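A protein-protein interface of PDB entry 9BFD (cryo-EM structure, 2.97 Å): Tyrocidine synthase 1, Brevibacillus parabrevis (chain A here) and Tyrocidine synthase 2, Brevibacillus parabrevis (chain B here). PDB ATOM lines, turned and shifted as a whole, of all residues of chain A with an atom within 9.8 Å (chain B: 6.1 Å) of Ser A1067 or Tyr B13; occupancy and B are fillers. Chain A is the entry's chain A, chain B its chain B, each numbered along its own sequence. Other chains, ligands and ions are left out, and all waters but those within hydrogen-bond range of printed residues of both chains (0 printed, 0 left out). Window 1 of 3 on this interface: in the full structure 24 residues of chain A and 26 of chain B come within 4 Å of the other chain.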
ATOM      1  N   GLU A 927      -0.826 -28.025   6.939  1.00  0.00           N
ATOM      2  CA  GLU A 927      -1.774 -27.271   7.748  1.00  0.00           C
ATOM      3  C   GLU A 927      -1.109 -26.129   8.503  1.00  0.00           C
ATOM      4  O   GLU A 927      -1.751 -25.097   8.744  1.00  0.00           O
ATOM      5  CB  GLU A 927      -2.503 -28.204   8.707  1.00  0.00           C
ATOM      6  CG  GLU A 927      -3.470 -29.131   7.998  1.00  0.00           C
ATOM      7  CD  GLU A 927      -4.602 -28.376   7.331  1.00  0.00           C
ATOM      8  OE1 GLU A 927      -4.915 -27.254   7.783  1.00  0.00           O
ATOM      9  OE2 GLU A 927      -5.175 -28.896   6.352  1.00  0.00           O
ATOM     10  N   ARG A1061      -7.035 -36.005   1.685  1.00  0.00           N
ATOM     11  CA  ARG A1061      -7.273 -34.599   1.972  1.00  0.00           C
ATOM     12  C   ARG A1061      -7.109 -34.299   3.455  1.00  0.00           C
ATOM     13  O   ARG A1061      -7.265 -35.168   4.315  1.00  0.00           O
ATOM     14  CB  ARG A1061      -8.669 -34.192   1.509  1.00  0.00           C
ATOM     15  CG  ARG A1061      -8.768 -33.925   0.022  1.00  0.00           C
ATOM     16  CD  ARG A1061     -10.196 -33.637  -0.381  1.00  0.00           C
ATOM     17  NE  ARG A1061     -11.035 -34.819  -0.223  1.00  0.00           N
ATOM     18  CZ  ARG A1061     -12.327 -34.864  -0.509  1.00  0.00           C
ATOM     19  NH1 ARG A1061     -12.967 -33.809  -0.984  1.00  0.00           N
ATOM     20  NH2 ARG A1061     -12.993 -35.998  -0.320  1.00  0.00           N
ATOM     21  N   THR A1062      -6.798 -33.043   3.745  1.00  0.00           N
ATOM     22  CA  THR A1062      -6.506 -32.545   5.076  1.00  0.00           C
ATOM     23  C   THR A1062      -7.548 -31.513   5.484  1.00  0.00           C
ATOM     24  O   THR A1062      -8.247 -30.951   4.632  1.00  0.00           O
ATOM     25  CB  THR A1062      -5.107 -31.918   5.119  1.00  0.00           C
ATOM     26  OG1 THR A1062      -5.085 -30.740   4.306  1.00  0.00           O
ATOM     27  CG2 THR A1062      -4.074 -32.897   4.596  1.00  0.00           C
ATOM     28  N   PRO A1063      -7.685 -31.243   6.782  1.00  0.00           N
ATOM     29  CA  PRO A1063      -8.838 -30.464   7.256  1.00  0.00           C
ATOM     30  C   PRO A1063      -9.037 -29.119   6.580  1.00  0.00           C
ATOM     31  O   PRO A1063     -10.168 -28.621   6.544  1.00  0.00           O
ATOM     32  CB  PRO A1063      -8.524 -30.285   8.744  1.00  0.00           C
ATOM     33  CG  PRO A1063      -7.741 -31.481   9.095  1.00  0.00           C
ATOM     34  CD  PRO A1063      -6.890 -31.778   7.897  1.00  0.00           C
ATOM     35  N   SER A1064      -7.980 -28.505   6.050  1.00  0.00           N
ATOM     36  CA  SER A1064      -8.143 -27.234   5.353  1.00  0.00           C
ATOM     37  C   SER A1064      -8.893 -27.372   4.041  1.00  0.00           C
ATOM     38  O   SER A1064      -9.395 -26.370   3.523  1.00  0.00           O
ATOM     39  CB  SER A1064      -6.780 -26.597   5.105  1.00  0.00           C
ATOM     40  OG  SER A1064      -5.907 -27.504   4.462  1.00  0.00           O
ATOM     41  N   ASP A1065      -8.981 -28.580   3.490  1.00  0.00           N
ATOM     42  CA  ASP A1065      -9.624 -28.778   2.199  1.00  0.00           C
ATOM     43  C   ASP A1065     -11.141 -28.648   2.241  1.00  0.00           C
ATOM     44  O   ASP A1065     -11.760 -28.599   1.173  1.00  0.00           O
ATOM     45  CB  ASP A1065      -9.249 -30.148   1.640  1.00  0.00           C
ATOM     46  CG  ASP A1065      -7.760 -30.309   1.454  1.00  0.00           C
ATOM     47  OD1 ASP A1065      -7.108 -29.341   1.011  1.00  0.00           O
ATOM     48  OD2 ASP A1065      -7.238 -31.404   1.748  1.00  0.00           O
ATOM     49  N   PHE A1066     -11.759 -28.591   3.423  1.00  0.00           N
ATOM     50  CA  PHE A1066     -13.188 -28.852   3.545  1.00  0.00           C
ATOM     51  C   PHE A1066     -14.019 -27.638   3.945  1.00  0.00           C
ATOM     52  O   PHE A1066     -15.166 -27.800   4.373  1.00  0.00           O
ATOM     53  CB  PHE A1066     -13.424 -29.995   4.529  1.00  0.00           C
ATOM     54  CG  PHE A1066     -13.040 -31.333   3.987  1.00  0.00           C
ATOM     55  CD1 PHE A1066     -13.679 -31.841   2.876  1.00  0.00           C
ATOM     56  CD2 PHE A1066     -12.051 -32.083   4.587  1.00  0.00           C
ATOM     57  CE1 PHE A1066     -13.333 -33.063   2.368  1.00  0.00           C
ATOM     58  CE2 PHE A1066     -11.705 -33.308   4.083  1.00  0.00           C
ATOM     59  CZ  PHE A1066     -12.346 -33.798   2.971  1.00  0.00           C
ATOM     60  N   SER A1067     -13.483 -26.428   3.818  1.00  0.00           N
ATOM     61  CA  SER A1067     -14.277 -25.202   3.928  1.00  0.00           C
ATOM     62  C   SER A1067     -15.052 -25.103   5.239  1.00  0.00           C
ATOM     63  O   SER A1067     -16.013 -24.336   5.334  1.00  0.00           O
ATOM     64  CB  SER A1067     -15.238 -25.053   2.742  1.00  0.00           C
ATOM     65  OG  SER A1067     -15.977 -26.240   2.519  1.00  0.00           O
ATOM     66  N   VAL A1068     -14.672 -25.871   6.256  1.00  0.00           N
ATOM     67  CA  VAL A1068     -15.214 -25.735   7.604  1.00  0.00           C
ATOM     68  C   VAL A1068     -14.150 -25.089   8.478  1.00  0.00           C
ATOM     69  O   VAL A1068     -13.036 -25.610   8.601  1.00  0.00           O
ATOM     70  CB  VAL A1068     -15.647 -27.091   8.179  1.00  0.00           C
ATOM     71  CG1 VAL A1068     -16.006 -26.951   9.642  1.00  0.00           C
ATOM     72  CG2 VAL A1068     -16.823 -27.644   7.396  1.00  0.00           C
ATOM     73  N   LYS A1069     -14.491 -23.956   9.086  1.00  0.00           N
ATOM     74  CA  LYS A1069     -13.524 -23.209   9.878  1.00  0.00           C
ATOM     75  C   LYS A1069     -13.170 -23.965  11.151  1.00  0.00           C
ATOM     76  O   LYS A1069     -14.050 -24.464  11.858  1.00  0.00           O
ATOM     77  CB  LYS A1069     -14.077 -21.828  10.225  1.00  0.00           C
ATOM     78  CG  LYS A1069     -13.893 -20.796   9.128  1.00  0.00           C
ATOM     79  CD  LYS A1069     -14.761 -21.113   7.924  1.00  0.00           C
ATOM     80  CE  LYS A1069     -14.660 -20.027   6.867  1.00  0.00           C
ATOM     81  NZ  LYS A1069     -15.761 -20.123   5.868  1.00  0.00           N
ATOM     82  N   GLY A1070     -11.874 -24.043  11.444  1.00  0.00           N
ATOM     83  CA  GLY A1070     -11.411 -24.653  12.674  1.00  0.00           C
ATOM     84  C   GLY A1070     -11.490 -26.160  12.718  1.00  0.00           C
ATOM     85  O   GLY A1070     -11.393 -26.742  13.801  1.00  0.00           O
ATOM     86  N   LEU A1071     -11.666 -26.810  11.575  1.00  0.00           N
ATOM     87  CA  LEU A1071     -11.672 -28.264  11.531  1.00  0.00           C
ATOM     88  C   LEU A1071     -10.294 -28.815  11.871  1.00  0.00           C
ATOM     89  O   LEU A1071      -9.269 -28.230  11.514  1.00  0.00           O
ATOM     90  CB  LEU A1071     -12.113 -28.747  10.152  1.00  0.00           C
ATOM     91  CG  LEU A1071     -12.530 -30.209  10.035  1.00  0.00           C
ATOM     92  CD1 LEU A1071     -13.829 -30.429  10.776  1.00  0.00           C
ATOM     93  CD2 LEU A1071     -12.673 -30.604   8.579  1.00  0.00           C
ATOM     94  N   MET A1076     -12.125 -34.260  11.625  1.00  0.00           N
ATOM     95  CA  MET A1076     -12.322 -34.625  10.229  1.00  0.00           C
ATOM     96  C   MET A1076     -12.426 -36.137  10.067  1.00  0.00           C
ATOM     97  O   MET A1076     -13.352 -36.642   9.417  1.00  0.00           O
ATOM     98  CB  MET A1076     -11.187 -34.070   9.371  1.00  0.00           C
ATOM     99  CG  MET A1076     -11.424 -34.227   7.881  1.00  0.00           C
ATOM    100  SD  MET A1076      -9.952 -33.978   6.882  1.00  0.00           S
ATOM    101  CE  MET A1076      -9.057 -35.486   7.224  1.00  0.00           C
ATOM    102  N   ILE A1079     -15.705 -37.390  11.523  1.00  0.00           N
ATOM    103  CA  ILE A1079     -16.792 -37.169  10.576  1.00  0.00           C
ATOM    104  C   ILE A1079     -16.763 -38.227   9.485  1.00  0.00           C
ATOM    105  O   ILE A1079     -17.796 -38.807   9.131  1.00  0.00           O
ATOM    106  CB  ILE A1079     -16.709 -35.750   9.987  1.00  0.00           C
ATOM    107  CG1 ILE A1079     -17.129 -34.712  11.028  1.00  0.00           C
ATOM    108  CG2 ILE A1079     -17.567 -35.639   8.745  1.00  0.00           C
ATOM    109  CD1 ILE A1079     -16.601 -33.324  10.756  1.00  0.00           C
ATOM    110  N   GLN B  10     -17.430 -34.149  -1.449  1.00  0.00           N
ATOM    111  CA  GLN B  10     -16.938 -32.972  -2.152  1.00  0.00           C
ATOM    112  C   GLN B  10     -16.524 -31.845  -1.212  1.00  0.00           C
ATOM    113  O   GLN B  10     -15.462 -31.242  -1.403  1.00  0.00           O
ATOM    114  CB  GLN B  10     -18.013 -32.462  -3.110  1.00  0.00           C
ATOM    115  CG  GLN B  10     -17.615 -31.253  -3.907  1.00  0.00           C
ATOM    116  CD  GLN B  10     -18.767 -30.687  -4.698  1.00  0.00           C
ATOM    117  OE1 GLN B  10     -19.518 -31.422  -5.331  1.00  0.00           O
ATOM    118  NE2 GLN B  10     -18.923 -29.372  -4.655  1.00  0.00           N
ATOM    119  N   ASP B  11     -17.339 -31.546  -0.203  1.00  0.00           N
ATOM    120  CA  ASP B  11     -17.067 -30.438   0.703  1.00  0.00           C
ATOM    121  C   ASP B  11     -17.907 -30.599   1.959  1.00  0.00           C
ATOM    122  O   ASP B  11     -18.814 -31.430   2.023  1.00  0.00           O
ATOM    123  CB  ASP B  11     -17.335 -29.087   0.039  1.00  0.00           C
ATOM    124  CG  ASP B  11     -16.063 -28.389  -0.393  1.00  0.00           C
ATOM    125  OD1 ASP B  11     -14.968 -28.883  -0.052  1.00  0.00           O
ATOM    126  OD2 ASP B  11     -16.158 -27.347  -1.072  1.00  0.00           O
ATOM    127  N   MET B  12     -17.585 -29.789   2.962  1.00  0.00           N
ATOM    128  CA  MET B  12     -18.409 -29.630   4.148  1.00  0.00           C
ATOM    129  C   MET B  12     -18.607 -28.147   4.436  1.00  0.00           C
ATOM    130  O   MET B  12     -17.792 -27.307   4.050  1.00  0.00           O
ATOM    131  CB  MET B  12     -17.773 -30.331   5.349  1.00  0.00           C
ATOM    132  CG  MET B  12     -17.429 -31.783   5.081  1.00  0.00           C
ATOM    133  SD  MET B  12     -16.612 -32.588   6.465  1.00  0.00           S
ATOM    134  CE  MET B  12     -16.253 -34.189   5.754  1.00  0.00           C
ATOM    135  N   TYR B  13     -19.700 -27.832   5.128  1.00  0.00           N
ATOM    136  CA  TYR B  13     -19.962 -26.475   5.592  1.00  0.00           C
ATOM    137  C   TYR B  13     -20.747 -26.538   6.894  1.00  0.00           C
ATOM    138  O   TYR B  13     -21.428 -27.525   7.183  1.00  0.00           O
ATOM    139  CB  TYR B  13     -20.748 -25.649   4.568  1.00  0.00           C
ATOM    140  CG  TYR B  13     -20.182 -25.650   3.173  1.00  0.00           C
ATOM    141  CD1 TYR B  13     -19.043 -24.927   2.862  1.00  0.00           C
ATOM    142  CD2 TYR B  13     -20.803 -26.356   2.157  1.00  0.00           C
ATOM    143  CE1 TYR B  13     -18.533 -24.917   1.580  1.00  0.00           C
ATOM    144  CE2 TYR B  13     -20.301 -26.360   0.879  1.00  0.00           C
ATOM    145  CZ  TYR B  13     -19.167 -25.637   0.593  1.00  0.00           C
ATOM    146  OH  TYR B  13     -18.658 -25.644  -0.685  1.00  0.00           O
ATOM    147  N   ALA B  14     -20.644 -25.472   7.682  1.00  0.00           N
ATOM    148  CA  ALA B  14     -21.632 -25.207   8.716  1.00  0.00           C
ATOM    149  C   ALA B  14     -22.971 -24.787   8.108  1.00  0.00           C
ATOM    150  O   ALA B  14     -23.049 -24.271   6.991  1.00  0.00           O
ATOM    151  CB  ALA B  14     -21.129 -24.124   9.667  1.00  0.00           C
ATOM    152  N   LEU B  15     -24.036 -25.020   8.872  1.00  0.00           N
ATOM    153  CA  LEU B  15     -25.389 -24.690   8.444  1.00  0.00           C
ATOM    154  C   LEU B  15     -25.650 -23.185   8.497  1.00  0.00           C
ATOM    155  O   LEU B  15     -25.131 -22.472   9.359  1.00  0.00           O
ATOM    156  CB  LEU B  15     -26.399 -25.417   9.329  1.00  0.00           C
ATOM    157  CG  LEU B  15     -26.706 -26.878   9.015  1.00  0.00           C
ATOM    158  CD1 LEU B  15     -25.451 -27.718   9.097  1.00  0.00           C
ATOM    159  CD2 LEU B  15     -27.747 -27.397   9.981  1.00  0.00           C
ATOM    160  N   ASP B  64     -25.507 -28.347  -5.814  1.00  0.00           N
ATOM    161  CA  ASP B  64     -24.882 -29.025  -4.687  1.00  0.00           C
ATOM    162  C   ASP B  64     -25.862 -29.218  -3.545  1.00  0.00           C
ATOM    163  O   ASP B  64     -25.734 -30.173  -2.770  1.00  0.00           O
ATOM    164  CB  ASP B  64     -23.667 -28.235  -4.205  1.00  0.00           C
ATOM    165  CG  ASP B  64     -22.601 -28.102  -5.271  1.00  0.00           C
ATOM    166  OD1 ASP B  64     -22.314 -29.107  -5.957  1.00  0.00           O
ATOM    167  OD2 ASP B  64     -22.049 -26.992  -5.424  1.00  0.00           O
ATOM    168  N   PRO B  78     -23.374 -29.195  13.741  1.00  0.00           N
ATOM    169  CA  PRO B  78     -24.024 -29.696  12.527  1.00  0.00           C
ATOM    170  C   PRO B  78     -23.252 -29.269  11.292  1.00  0.00           C
ATOM    171  O   PRO B  78     -22.815 -28.123  11.178  1.00  0.00           O
ATOM    172  CB  PRO B  78     -25.413 -29.054  12.577  1.00  0.00           C
ATOM    173  CG  PRO B  78     -25.619 -28.713  14.009  1.00  0.00           C
ATOM    174  CD  PRO B  78     -24.273 -28.347  14.536  1.00  0.00           C
ATOM    175  N   LEU B  79     -23.089 -30.197  10.360  1.00  0.00           N
ATOM    176  CA  LEU B  79     -22.432 -29.906   9.097  1.00  0.00           C
ATOM    177  C   LEU B  79     -23.344 -30.239   7.928  1.00  0.00           C
ATOM    178  O   LEU B  79     -24.091 -31.220   7.968  1.00  0.00           O
ATOM    179  CB  LEU B  79     -21.129 -30.690   8.960  1.00  0.00           C
ATOM    180  CG  LEU B  79     -19.991 -30.342   9.912  1.00  0.00           C
ATOM    181  CD1 LEU B  79     -18.776 -31.172   9.572  1.00  0.00           C
ATOM    182  CD2 LEU B  79     -19.666 -28.864   9.838  1.00  0.00           C
ATOM    183  N   GLN B  80     -23.278 -29.411   6.892  1.00  0.00           N
ATOM    184  CA  GLN B  80     -23.585 -29.864   5.547  1.00  0.00           C
ATOM    185  C   GLN B  80     -22.449 -30.749   5.059  1.00  0.00           C
ATOM    186  O   GLN B  80     -21.274 -30.391   5.193  1.00  0.00           O
ATOM    187  CB  GLN B  80     -23.750 -28.671   4.610  1.00  0.00           C
ATOM    188  CG  GLN B  80     -24.939 -27.785   4.890  1.00  0.00           C
ATOM    189  CD  GLN B  80     -25.217 -26.836   3.745  1.00  0.00           C
ATOM    190  OE1 GLN B  80     -25.665 -25.711   3.950  1.00  0.00           O
ATOM    191  NE2 GLN B  80     -24.947 -27.286   2.529  1.00  0.00           N
ATOM    192  N   VAL B  81     -22.783 -31.902   4.495  1.00  0.00           N
ATOM    193  CA  VAL B  81     -21.833 -32.688   3.720  1.00  0.00           C
ATOM    194  C   VAL B  81     -22.366 -32.801   2.303  1.00  0.00           C
ATOM    195  O   VAL B  81     -23.472 -33.311   2.089  1.00  0.00           O
ATOM    196  CB  VAL B  81     -21.600 -34.075   4.337  1.00  0.00           C
ATOM    197  CG1 VAL B  81     -20.601 -34.855   3.516  1.00  0.00           C
ATOM    198  CG2 VAL B  81     -21.109 -33.932   5.756  1.00  0.00           C
ATOM    199  N   VAL B  82     -21.589 -32.328   1.341  1.00  0.00           N
ATOM    200  CA  VAL B  82     -21.966 -32.372  -0.063  1.00  0.00           C
ATOM    201  C   VAL B  82     -21.302 -33.594  -0.677  1.00  0.00           C
ATOM    202  O   VAL B  82     -20.073 -33.654  -0.790  1.00  0.00           O
ATOM    203  CB  VAL B  82     -21.567 -31.085  -0.796  1.00  0.00           C
ATOM    204  CG1 VAL B  82     -21.992 -31.145  -2.246  1.00  0.00           C
ATOM    205  CG2 VAL B  82     -22.183 -29.879  -0.116  1.00  0.00           C
ATOM    206  N   SER B 184     -22.165 -21.436  -1.033  1.00  0.00           N
ATOM    207  CA  SER B 184     -21.036 -21.120  -0.174  1.00  0.00           C
ATOM    208  C   SER B 184     -20.709 -19.636  -0.184  1.00  0.00           C
ATOM    209  O   SER B 184     -20.111 -19.142   0.777  1.00  0.00           O
ATOM    210  CB  SER B 184     -19.810 -21.928  -0.599  1.00  0.00           C
ATOM    211  OG  SER B 184     -19.361 -21.536  -1.885  1.00  0.00           O
ATOM    212  N   ILE B 187     -22.836 -18.585   2.676  1.00  0.00           N
ATOM    213  CA  ILE B 187     -22.239 -19.041   3.934  1.00  0.00           C
ATOM    214  C   ILE B 187     -21.052 -18.159   4.329  1.00  0.00           C
ATOM    215  O   ILE B 187     -20.942 -17.697   5.477  1.00  0.00           O
ATOM    216  CB  ILE B 187     -21.831 -20.519   3.824  1.00  0.00           C
ATOM    217  CG1 ILE B 187     -23.070 -21.407   3.752  1.00  0.00           C
ATOM    218  CG2 ILE B 187     -20.953 -20.917   5.000  1.00  0.00           C
ATOM    219  CD1 ILE B 187     -22.805 -22.776   3.179  1.00  0.00           C
ATOM    220  N   ASN B 188     -20.168 -17.872   3.371  1.00  0.00           N
ATOM    221  CA  ASN B 188     -19.031 -17.005   3.656  1.00  0.00           C
ATOM    222  C   ASN B 188     -19.480 -15.608   4.051  1.00  0.00           C
ATOM    223  O   ASN B 188     -18.940 -15.018   4.994  1.00  0.00           O
ATOM    224  CB  ASN B 188     -18.104 -16.941   2.442  1.00  0.00           C
ATOM    225  CG  ASN B 188     -17.171 -18.134   2.357  1.00  0.00           C
ATOM    226  OD1 ASN B 188     -16.239 -18.266   3.149  1.00  0.00           O
ATOM    227  ND2 ASN B 188     -17.414 -19.005   1.386  1.00  0.00           N
ATOM    228  N   GLU B 191     -20.576 -15.453   7.497  1.00  0.00           N
ATOM    229  CA  GLU B 191     -19.500 -15.469   8.483  1.00  0.00           C
ATOM    230  C   GLU B 191     -18.719 -14.161   8.525  1.00  0.00           C
ATOM    231  O   GLU B 191     -18.160 -13.815   9.571  1.00  0.00           O
ATOM    232  CB  GLU B 191     -18.547 -16.631   8.205  1.00  0.00           C
ATOM    233  CG  GLU B 191     -19.175 -18.002   8.383  1.00  0.00           C
ATOM    234  CD  GLU B 191     -18.213 -19.128   8.065  1.00  0.00           C
ATOM    235  OE1 GLU B 191     -17.423 -18.985   7.109  1.00  0.00           O
ATOM    236  OE2 GLU B 191     -18.243 -20.155   8.776  1.00  0.00           O
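The side-chain carboxylate of Asp A1065 is in hydrogen-bond range of the backbone NH of Thr A1062 (2.6 Å). O of Ser B184 sits at hydrogen-bond distance from ND2 of Asn B188. The side-chain hydroxyl (OH) of Tyr B13 sits at hydrogen-bond distance from the side-chain carboxylate (OD2) of Asp B11. O of Tyr B13 is in hydrogen-bond range of N of Gln B80, at 2.7 Å. The backbone carbonyl oxygen (O) of Val B82 is in hydrogen-bond range of the backbone NH (N) of Gln B10. The backbone carbonyl oxygen (O) of Asp B11 lies within hydrogen-bond range of the backbone NH (N) of Val B82, 3.0 Å away.
Of the printed residues of chain B, Arg A1061 touches Gln B10. Of chain B, only Asp B11, Met B12 and Tyr B13 come within 4 Å of Ser A1067. Of chain A, only Ser A1067 (3.0 Å) and Val A1068 (3.7 Å) come within 4 Å of Tyr B13. Of chain A, only Val A1068 and Ile A1079 come within 4 Å of Leu B79. Gln B80 touches none of the printed residues of chain A. Of the printed residues of chain A, Asn B188 touches Lys A1069. Of the printed residues of chain A, Glu B191 touches Lys A1069 (2.4 Å).
The backbone carbonyl oxygen of Phe A1066 lies within hydrogen-bond range of the backbone NH of Met B12, at 3.4 Å. The side-chain amino group of Lys A1069 lies within salt-bridge range of the side-chain carboxylate of Glu B191. The backbone carbonyl oxygen (O) of Asp A1065 lies close to the side-chain carboxylate (OD1) of Asp B11 (3.4 Å). OG of Ser A1067 sits at hydrogen-bond distance from O of Met B12, 2.6 Å away. The side-chain amino group (NZ) of Lys A1069 sits at hydrogen-bond distance from the side-chain amide oxygen (OD1) of Asn B188.
NH1 of Arg A1061 touches O of Gln B10, at 3.6 Å. Ser A1067 touches Asp B11. Tyr B13 touches Ser A1067. Val A1068 touches Met B12. Val A1068 touches Tyr B13. Val A1068 touches Leu B79 (CG2 to CD2, 3.9 Å). Ile A1079 touches Met B12 (CG2 to CE, 3.6 Å). CD1 of Leu B79 touches CD1 of Ile A1079, 3.3 Å away.
Hydrophobic or aromatic side chains of chain A within 4 Å of the printed part of chain B: Val A1068 and Ile A1079. Among the printed residues, Asp or Glu carboxylates within 4 Å of a Lys or Arg side-chain nitrogen of the other chain: Lys A1069 with Glu B191.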
